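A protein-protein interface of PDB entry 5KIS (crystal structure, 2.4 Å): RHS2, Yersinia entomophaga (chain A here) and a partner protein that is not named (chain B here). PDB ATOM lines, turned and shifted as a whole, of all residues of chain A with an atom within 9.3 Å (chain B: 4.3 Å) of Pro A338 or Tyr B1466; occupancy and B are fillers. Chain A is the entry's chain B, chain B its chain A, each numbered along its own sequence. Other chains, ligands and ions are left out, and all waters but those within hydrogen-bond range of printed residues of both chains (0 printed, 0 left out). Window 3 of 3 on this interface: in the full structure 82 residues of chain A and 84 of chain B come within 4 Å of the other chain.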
ATOM      1  N   PHE A   6       7.718  27.834 -17.376  1.00  0.00           N
ATOM      2  CA  PHE A   6       7.214  29.107 -16.859  1.00  0.00           C
ATOM      3  C   PHE A   6       7.839  30.338 -17.546  1.00  0.00           C
ATOM      4  O   PHE A   6       7.490  31.466 -17.199  1.00  0.00           O
ATOM      5  CB  PHE A   6       7.414  29.155 -15.331  1.00  0.00           C
ATOM      6  CG  PHE A   6       6.898  27.923 -14.609  1.00  0.00           C
ATOM      7  CD1 PHE A   6       5.527  27.657 -14.553  1.00  0.00           C
ATOM      8  CD2 PHE A   6       7.778  27.024 -13.996  1.00  0.00           C
ATOM      9  CE1 PHE A   6       5.041  26.527 -13.902  1.00  0.00           C
ATOM     10  CE2 PHE A   6       7.296  25.893 -13.347  1.00  0.00           C
ATOM     11  CZ  PHE A   6       5.926  25.644 -13.300  1.00  0.00           C
ATOM     12  N   GLU A 305      11.416  26.891   6.603  1.00  0.00           N
ATOM     13  CA  GLU A 305      12.479  27.481   5.792  1.00  0.00           C
ATOM     14  C   GLU A 305      12.791  28.867   6.380  1.00  0.00           C
ATOM     15  O   GLU A 305      11.870  29.672   6.585  1.00  0.00           O
ATOM     16  CB  GLU A 305      12.024  27.594   4.325  1.00  0.00           C
ATOM     17  CG  GLU A 305      13.136  27.979   3.352  1.00  0.00           C
ATOM     18  CD  GLU A 305      12.920  27.455   1.938  1.00  0.00           C
ATOM     19  OE1 GLU A 305      11.857  27.719   1.344  1.00  0.00           O
ATOM     20  OE2 GLU A 305      13.832  26.780   1.419  1.00  0.00           O
ATOM     21  N   GLU A 307      14.257  31.457   5.117  1.00  0.00           N
ATOM     22  CA  GLU A 307      14.169  32.537   4.156  1.00  0.00           C
ATOM     23  C   GLU A 307      12.727  32.929   3.907  1.00  0.00           C
ATOM     24  O   GLU A 307      12.375  34.098   4.025  1.00  0.00           O
ATOM     25  CB  GLU A 307      14.837  32.124   2.839  1.00  0.00           C
ATOM     26  CG  GLU A 307      16.324  31.798   2.976  1.00  0.00           C
ATOM     27  CD  GLU A 307      16.623  30.339   3.294  1.00  0.00           C
ATOM     28  OE1 GLU A 307      15.790  29.664   3.939  1.00  0.00           O
ATOM     29  OE2 GLU A 307      17.711  29.865   2.902  1.00  0.00           O
ATOM     30  N   THR A 308      11.905  31.939   3.575  1.00  0.00           N
ATOM     31  CA  THR A 308      10.513  32.137   3.146  1.00  0.00           C
ATOM     32  C   THR A 308       9.471  31.929   4.242  1.00  0.00           C
ATOM     33  O   THR A 308       8.303  32.274   4.057  1.00  0.00           O
ATOM     34  CB  THR A 308      10.146  31.135   2.037  1.00  0.00           C
ATOM     35  OG1 THR A 308      10.145  29.806   2.574  1.00  0.00           O
ATOM     36  CG2 THR A 308      11.138  31.211   0.873  1.00  0.00           C
ATOM     37  N   ARG A 310       8.128  29.200   5.004  1.00  0.00           N
ATOM     38  CA  ARG A 310       7.202  28.166   4.573  1.00  0.00           C
ATOM     39  C   ARG A 310       7.375  26.973   5.485  1.00  0.00           C
ATOM     40  O   ARG A 310       8.490  26.683   5.930  1.00  0.00           O
ATOM     41  CB  ARG A 310       7.471  27.748   3.137  1.00  0.00           C
ATOM     42  CG  ARG A 310       7.140  28.829   2.137  1.00  0.00           C
ATOM     43  CD  ARG A 310       7.778  28.548   0.789  1.00  0.00           C
ATOM     44  NE  ARG A 310       7.475  29.603  -0.172  1.00  0.00           N
ATOM     45  CZ  ARG A 310       7.932  29.656  -1.427  1.00  0.00           C
ATOM     46  NH1 ARG A 310       8.740  28.711  -1.924  1.00  0.00           N
ATOM     47  NH2 ARG A 310       7.570  30.671  -2.201  1.00  0.00           N
ATOM     48  N   GLU A 335       8.692  20.044  -0.088  1.00  0.00           N
ATOM     49  CA  GLU A 335       9.601  20.685  -1.015  1.00  0.00           C
ATOM     50  C   GLU A 335       8.744  21.561  -1.903  1.00  0.00           C
ATOM     51  O   GLU A 335       7.808  21.075  -2.543  1.00  0.00           O
ATOM     52  CB  GLU A 335      10.336  19.646  -1.853  1.00  0.00           C
ATOM     53  CG  GLU A 335      11.266  18.739  -1.047  1.00  0.00           C
ATOM     54  CD  GLU A 335      12.015  17.711  -1.897  1.00  0.00           C
ATOM     55  OE1 GLU A 335      12.372  18.004  -3.073  1.00  0.00           O
ATOM     56  OE2 GLU A 335      12.261  16.598  -1.376  1.00  0.00           O
ATOM     57  N   TYR A 336       9.048  22.859  -1.916  1.00  0.00           N
ATOM     58  CA  TYR A 336       8.285  23.835  -2.689  1.00  0.00           C
ATOM     59  C   TYR A 336       9.043  24.252  -3.940  1.00  0.00           C
ATOM     60  O   TYR A 336      10.276  24.229  -3.968  1.00  0.00           O
ATOM     61  CB  TYR A 336       8.009  25.070  -1.845  1.00  0.00           C
ATOM     62  CG  TYR A 336       7.203  24.785  -0.614  1.00  0.00           C
ATOM     63  CD1 TYR A 336       5.810  24.763  -0.659  1.00  0.00           C
ATOM     64  CD2 TYR A 336       7.825  24.533   0.598  1.00  0.00           C
ATOM     65  CE1 TYR A 336       5.060  24.500   0.480  1.00  0.00           C
ATOM     66  CE2 TYR A 336       7.090  24.273   1.741  1.00  0.00           C
ATOM     67  CZ  TYR A 336       5.710  24.251   1.680  1.00  0.00           C
ATOM     68  OH  TYR A 336       4.978  23.984   2.816  1.00  0.00           O
ATOM     69  N   ASP A 337       8.297  24.647  -4.964  1.00  0.00           N
ATOM     70  CA  ASP A 337       8.879  25.354  -6.093  1.00  0.00           C
ATOM     71  C   ASP A 337       9.016  26.836  -5.664  1.00  0.00           C
ATOM     72  O   ASP A 337       8.541  27.205  -4.585  1.00  0.00           O
ATOM     73  CB  ASP A 337       8.042  25.122  -7.377  1.00  0.00           C
ATOM     74  CG  ASP A 337       6.792  25.985  -7.457  1.00  0.00           C
ATOM     75  OD1 ASP A 337       6.394  26.609  -6.453  1.00  0.00           O
ATOM     76  OD2 ASP A 337       6.193  26.027  -8.547  1.00  0.00           O
ATOM     77  N   PRO A 338       9.647  27.688  -6.494  1.00  0.00           N
ATOM     78  CA  PRO A 338       9.937  29.051  -6.038  1.00  0.00           C
ATOM     79  C   PRO A 338       8.734  29.872  -5.548  1.00  0.00           C
ATOM     80  O   PRO A 338       8.853  30.518  -4.515  1.00  0.00           O
ATOM     81  CB  PRO A 338      10.587  29.699  -7.262  1.00  0.00           C
ATOM     82  CG  PRO A 338      11.174  28.565  -8.037  1.00  0.00           C
ATOM     83  CD  PRO A 338      10.227  27.422  -7.824  1.00  0.00           C
ATOM     84  N   VAL A 339       7.596  29.823  -6.248  1.00  0.00           N
ATOM     85  CA  VAL A 339       6.384  30.551  -5.802  1.00  0.00           C
ATOM     86  C   VAL A 339       5.596  29.892  -4.670  1.00  0.00           C
ATOM     87  O   VAL A 339       4.636  30.487  -4.163  1.00  0.00           O
ATOM     88  CB  VAL A 339       5.381  30.859  -6.937  1.00  0.00           C
ATOM     89  CG1 VAL A 339       6.030  31.730  -8.002  1.00  0.00           C
ATOM     90  CG2 VAL A 339       4.765  29.581  -7.506  1.00  0.00           C
ATOM     91  N   GLY A 340       5.963  28.670  -4.290  1.00  0.00           N
ATOM     92  CA  GLY A 340       5.368  28.012  -3.114  1.00  0.00           C
ATOM     93  C   GLY A 340       4.290  26.976  -3.381  1.00  0.00           C
ATOM     94  O   GLY A 340       3.456  26.711  -2.508  1.00  0.00           O
ATOM     95  N   ASN A 341       4.299  26.402  -4.581  1.00  0.00           N
ATOM     96  CA  ASN A 341       3.502  25.216  -4.887  1.00  0.00           C
ATOM     97  C   ASN A 341       4.278  24.027  -4.334  1.00  0.00           C
ATOM     98  O   ASN A 341       5.516  24.043  -4.297  1.00  0.00           O
ATOM     99  CB  ASN A 341       3.281  25.061  -6.396  1.00  0.00           C
ATOM    100  CG  ASN A 341       2.543  26.245  -7.007  1.00  0.00           C
ATOM    101  OD1 ASN A 341       1.515  26.684  -6.505  1.00  0.00           O
ATOM    102  ND2 ASN A 341       3.067  26.767  -8.100  1.00  0.00           N
ATOM    103  N   VAL A 342       3.544  23.007  -3.895  1.00  0.00           N
ATOM    104  CA  VAL A 342       4.145  21.833  -3.283  1.00  0.00           C
ATOM    105  C   VAL A 342       4.536  20.874  -4.394  1.00  0.00           C
ATOM    106  O   VAL A 342       3.675  20.392  -5.116  1.00  0.00           O
ATOM    107  CB  VAL A 342       3.165  21.143  -2.323  1.00  0.00           C
ATOM    108  CG1 VAL A 342       3.770  19.852  -1.767  1.00  0.00           C
ATOM    109  CG2 VAL A 342       2.765  22.103  -1.202  1.00  0.00           C
ATOM    110  N   LEU A 343       5.832  20.623  -4.543  1.00  0.00           N
ATOM    111  CA  LEU A 343       6.317  19.698  -5.558  1.00  0.00           C
ATOM    112  C   LEU A 343       6.390  18.264  -5.017  1.00  0.00           C
ATOM    113  O   LEU A 343       6.018  17.318  -5.722  1.00  0.00           O
ATOM    114  CB  LEU A 343       7.683  20.147  -6.107  1.00  0.00           C
ATOM    115  CG  LEU A 343       7.731  21.429  -6.964  1.00  0.00           C
ATOM    116  CD1 LEU A 343       9.127  21.619  -7.558  1.00  0.00           C
ATOM    117  CD2 LEU A 343       6.687  21.472  -8.077  1.00  0.00           C
ATOM    118  N   TYR A 372      -0.454  27.380 -12.278  1.00  0.00           N
ATOM    119  CA  TYR A 372      -0.338  26.727 -10.968  1.00  0.00           C
ATOM    120  C   TYR A 372      -1.564  25.909 -10.583  1.00  0.00           C
ATOM    121  O   TYR A 372      -1.964  25.868  -9.410  1.00  0.00           O
ATOM    122  CB  TYR A 372       0.073  27.737  -9.893  1.00  0.00           C
ATOM    123  CG  TYR A 372       1.197  28.639 -10.367  1.00  0.00           C
ATOM    124  CD1 TYR A 372       2.302  28.117 -11.071  1.00  0.00           C
ATOM    125  CD2 TYR A 372       1.158  30.013 -10.136  1.00  0.00           C
ATOM    126  CE1 TYR A 372       3.326  28.936 -11.522  1.00  0.00           C
ATOM    127  CE2 TYR A 372       2.186  30.840 -10.576  1.00  0.00           C
ATOM    128  CZ  TYR A 372       3.268  30.299 -11.270  1.00  0.00           C
ATOM    129  OH  TYR A 372       4.289  31.097 -11.724  1.00  0.00           O
ATOM    130  N   TRP A 683      -3.020  25.238  -0.990  1.00  0.00           N
ATOM    131  CA  TRP A 683      -4.056  26.104  -0.381  1.00  0.00           C
ATOM    132  C   TRP A 683      -5.229  25.315   0.231  1.00  0.00           C
ATOM    133  O   TRP A 683      -5.433  24.131  -0.044  1.00  0.00           O
ATOM    134  CB  TRP A 683      -4.578  27.176  -1.370  1.00  0.00           C
ATOM    135  CG  TRP A 683      -3.509  27.926  -2.191  1.00  0.00           C
ATOM    136  CD1 TRP A 683      -3.573  28.210  -3.528  1.00  0.00           C
ATOM    137  CD2 TRP A 683      -2.239  28.462  -1.731  1.00  0.00           C
ATOM    138  NE1 TRP A 683      -2.440  28.883  -3.930  1.00  0.00           N
ATOM    139  CE2 TRP A 683      -1.604  29.051  -2.856  1.00  0.00           C
ATOM    140  CE3 TRP A 683      -1.576  28.498  -0.485  1.00  0.00           C
ATOM    141  CZ2 TRP A 683      -0.333  29.674  -2.775  1.00  0.00           C
ATOM    142  CZ3 TRP A 683      -0.306  29.121  -0.406  1.00  0.00           C
ATOM    143  CH2 TRP A 683       0.294  29.698  -1.547  1.00  0.00           C
ATOM    144  N   VAL B1460      11.782  42.791  -7.001  1.00  0.00           N
ATOM    145  CA  VAL B1460      12.006  42.286  -5.650  1.00  0.00           C
ATOM    146  C   VAL B1460      12.974  41.126  -5.740  1.00  0.00           C
ATOM    147  O   VAL B1460      12.770  40.233  -6.553  1.00  0.00           O
ATOM    148  CB  VAL B1460      10.701  41.762  -5.012  1.00  0.00           C
ATOM    149  CG1 VAL B1460      10.967  41.206  -3.615  1.00  0.00           C
ATOM    150  CG2 VAL B1460       9.640  42.857  -4.967  1.00  0.00           C
ATOM    151  N   ILE B1461      14.022  41.145  -4.920  1.00  0.00           N
ATOM    152  CA  ILE B1461      14.928  40.007  -4.772  1.00  0.00           C
ATOM    153  C   ILE B1461      14.597  39.373  -3.441  1.00  0.00           C
ATOM    154  O   ILE B1461      14.843  39.969  -2.406  1.00  0.00           O
ATOM    155  CB  ILE B1461      16.421  40.411  -4.753  1.00  0.00           C
ATOM    156  CG1 ILE B1461      16.762  41.413  -5.870  1.00  0.00           C
ATOM    157  CG2 ILE B1461      17.311  39.177  -4.829  1.00  0.00           C
ATOM    158  CD1 ILE B1461      16.434  40.939  -7.264  1.00  0.00           C
ATOM    159  N   THR B1462      14.042  38.165  -3.468  1.00  0.00           N
ATOM    160  CA  THR B1462      13.635  37.475  -2.238  1.00  0.00           C
ATOM    161  C   THR B1462      14.880  37.013  -1.486  1.00  0.00           C
ATOM    162  O   THR B1462      15.946  36.827  -2.090  1.00  0.00           O
ATOM    163  CB  THR B1462      12.728  36.254  -2.503  1.00  0.00           C
ATOM    164  OG1 THR B1462      13.505  35.158  -3.003  1.00  0.00           O
ATOM    165  CG2 THR B1462      11.615  36.586  -3.493  1.00  0.00           C
ATOM    166  N   LYS B1464      15.698  34.175  -0.394  1.00  0.00           N
ATOM    167  CA  LYS B1464      16.185  32.897  -0.929  1.00  0.00           C
ATOM    168  C   LYS B1464      17.038  33.093  -2.182  1.00  0.00           C
ATOM    169  O   LYS B1464      17.857  32.244  -2.491  1.00  0.00           O
ATOM    170  CB  LYS B1464      15.000  31.964  -1.249  1.00  0.00           C
ATOM    171  CG  LYS B1464      15.065  30.580  -0.614  1.00  0.00           C
ATOM    172  CD  LYS B1464      15.832  29.567  -1.456  1.00  0.00           C
ATOM    173  CE  LYS B1464      15.481  28.138  -1.059  1.00  0.00           C
ATOM    174  NZ  LYS B1464      14.107  27.723  -1.475  1.00  0.00           N
ATOM    175  N   GLY B1465      16.833  34.198  -2.899  1.00  0.00           N
ATOM    176  CA  GLY B1465      17.592  34.526  -4.106  1.00  0.00           C
ATOM    177  C   GLY B1465      16.757  34.782  -5.349  1.00  0.00           C
ATOM    178  O   GLY B1465      17.302  35.224  -6.345  1.00  0.00           O
ATOM    179  N   TYR B1466      15.446  34.521  -5.305  1.00  0.00           N
ATOM    180  CA  TYR B1466      14.566  34.643  -6.492  1.00  0.00           C
ATOM    181  C   TYR B1466      14.174  36.088  -6.806  1.00  0.00           C
ATOM    182  O   TYR B1466      14.546  36.998  -6.074  1.00  0.00           O
ATOM    183  CB  TYR B1466      13.318  33.758  -6.323  1.00  0.00           C
ATOM    184  CG  TYR B1466      13.665  32.290  -6.343  1.00  0.00           C
ATOM    185  CD1 TYR B1466      14.065  31.676  -7.539  1.00  0.00           C
ATOM    186  CD2 TYR B1466      13.629  31.515  -5.177  1.00  0.00           C
ATOM    187  CE1 TYR B1466      14.403  30.336  -7.587  1.00  0.00           C
ATOM    188  CE2 TYR B1466      13.968  30.167  -5.211  1.00  0.00           C
ATOM    189  CZ  TYR B1466      14.354  29.581  -6.423  1.00  0.00           C
ATOM    190  OH  TYR B1466      14.695  28.247  -6.507  1.00  0.00           O
ATOM    191  N   ARG B1467      13.453  36.291  -7.910  1.00  0.00           N
ATOM    192  CA  ARG B1467      13.039  37.625  -8.335  1.00  0.00           C
ATOM    193  C   ARG B1467      11.570  37.710  -8.722  1.00  0.00           C
ATOM    194  O   ARG B1467      11.035  36.821  -9.378  1.00  0.00           O
ATOM    195  CB  ARG B1467      13.862  38.087  -9.532  1.00  0.00           C
ATOM    196  CG  ARG B1467      15.361  38.160  -9.302  1.00  0.00           C
ATOM    197  CD  ARG B1467      16.034  38.911 -10.452  1.00  0.00           C
ATOM    198  NE  ARG B1467      17.499  38.804 -10.405  1.00  0.00           N
ATOM    199  CZ  ARG B1467      18.373  39.806 -10.249  1.00  0.00           C
ATOM    200  NH1 ARG B1467      17.985  41.073 -10.120  1.00  0.00           N
ATOM    201  NH2 ARG B1467      19.676  39.531 -10.226  1.00  0.00           N
ATOM    202  N   GLU B1482       8.260  34.448  -9.197  1.00  0.00           N
ATOM    203  CA  GLU B1482       9.558  33.812  -8.972  1.00  0.00           C
ATOM    204  C   GLU B1482       9.841  32.645  -9.913  1.00  0.00           C
ATOM    205  O   GLU B1482      11.000  32.390 -10.237  1.00  0.00           O
ATOM    206  CB  GLU B1482       9.700  33.389  -7.512  1.00  0.00           C
ATOM    207  CG  GLU B1482       9.689  34.560  -6.530  1.00  0.00           C
ATOM    208  CD  GLU B1482       8.335  34.829  -5.886  1.00  0.00           C
ATOM    209  OE1 GLU B1482       7.287  34.729  -6.571  1.00  0.00           O
ATOM    210  OE2 GLU B1482       8.341  35.156  -4.677  1.00  0.00           O
ATOM    211  N   ASN B1483       8.786  31.965 -10.370  1.00  0.00           N
ATOM    212  CA  ASN B1483       8.912  30.889 -11.358  1.00  0.00           C
ATOM    213  C   ASN B1483       9.207  31.456 -12.749  1.00  0.00           C
ATOM    214  O   ASN B1483      10.078  30.943 -13.449  1.00  0.00           O
ATOM    215  CB  ASN B1483       7.643  30.023 -11.411  1.00  0.00           C
ATOM    216  CG  ASN B1483       7.537  29.034 -10.251  1.00  0.00           C
ATOM    217  OD1 ASN B1483       7.950  29.307  -9.120  1.00  0.00           O
ATOM    218  ND2 ASN B1483       6.948  27.885 -10.530  1.00  0.00           N
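The side-chain amino group (NZ) of Lys B1464 lies within salt-bridge range of the side-chain carboxylate (OE2) of Glu A305. The side-chain amide nitrogen (ND2) of Asn B1483 is in hydrogen-bond range of the side-chain carboxylate (OD2) of Asp A337 (2.8 Å). N of Val A339 lies within hydrogen-bond range of OD1 of Asn B1483 (2.9 Å).
OG1 of Thr B1462 sits at hydrogen-bond distance from N of Tyr B1466. OE1 of Glu A305 is in hydrogen-bond range of OG1 of Thr A308 (3.0 Å). The backbone carbonyl oxygen of Asp A337 lies within hydrogen-bond range of the guanidinium group of Arg A310, at 3.1 Å. The guanidinium group (NH2) of Arg A310 is in hydrogen-bond range of the backbone carbonyl oxygen (O) of Pro A338 (2.7 Å). The side-chain carboxylate (OD1) of Asp A337 sits close to the backbone NH (N) of Val A339. The backbone NH (N) of Asn A341 sits at hydrogen-bond distance from the side-chain carboxylate (OD1) of Asp A337 (2.8 Å).
Among the printed residues, pairs that only touch across the chains: Phe A6 with Asn B1483 (3.5 Å), Glu A307 with Lys B1464 (3.8 Å), Pro A338 with Tyr B1466 (3.7 Å), Pro A338 with Glu B1482 (3.8 Å), Pro A338 with Asn B1483 (3.2 Å), Val A339 with Glu B1482 (3.6 Å) and Tyr A372 with Asn B1483 (3.5 Å).
Thr A308 touches none of the printed residues of chain B. Of the printed residues of chain B, Asp A337 touches Asn B1483. Pro A338 touches three residues of chain B. Printed residues of chain B within 4 Å of Tyr A372: Asn B1483. No residue of chain A comes within 4 Å of Ile B1461. No residue of chain A comes within 4 Å of Thr B1462. Of chain A, only Glu A305 and Glu A307 come within 4 Å of Lys B1464. Gly B1465 touches none of the printed residues of chain A. Tyr B1466 touches just one residue of chain A: Pro A338. The nearest printed residue of chain B that does not touch Pro A338 is Lys B1464 (6.3 Å). The nearest residue of chain A that does not touch Tyr B1466 is Asp A337 (5.9 Å). The nearest printed residue of chain B that does not touch Asp A337 is Tyr B1466 (5.9 Å).
Printed residues of chain B that touch a printed residue of chain A: Lys B1464, Tyr B1466, Glu B1482 and Asn B1483. Among the printed residues, 10 pairs touch across the chains.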
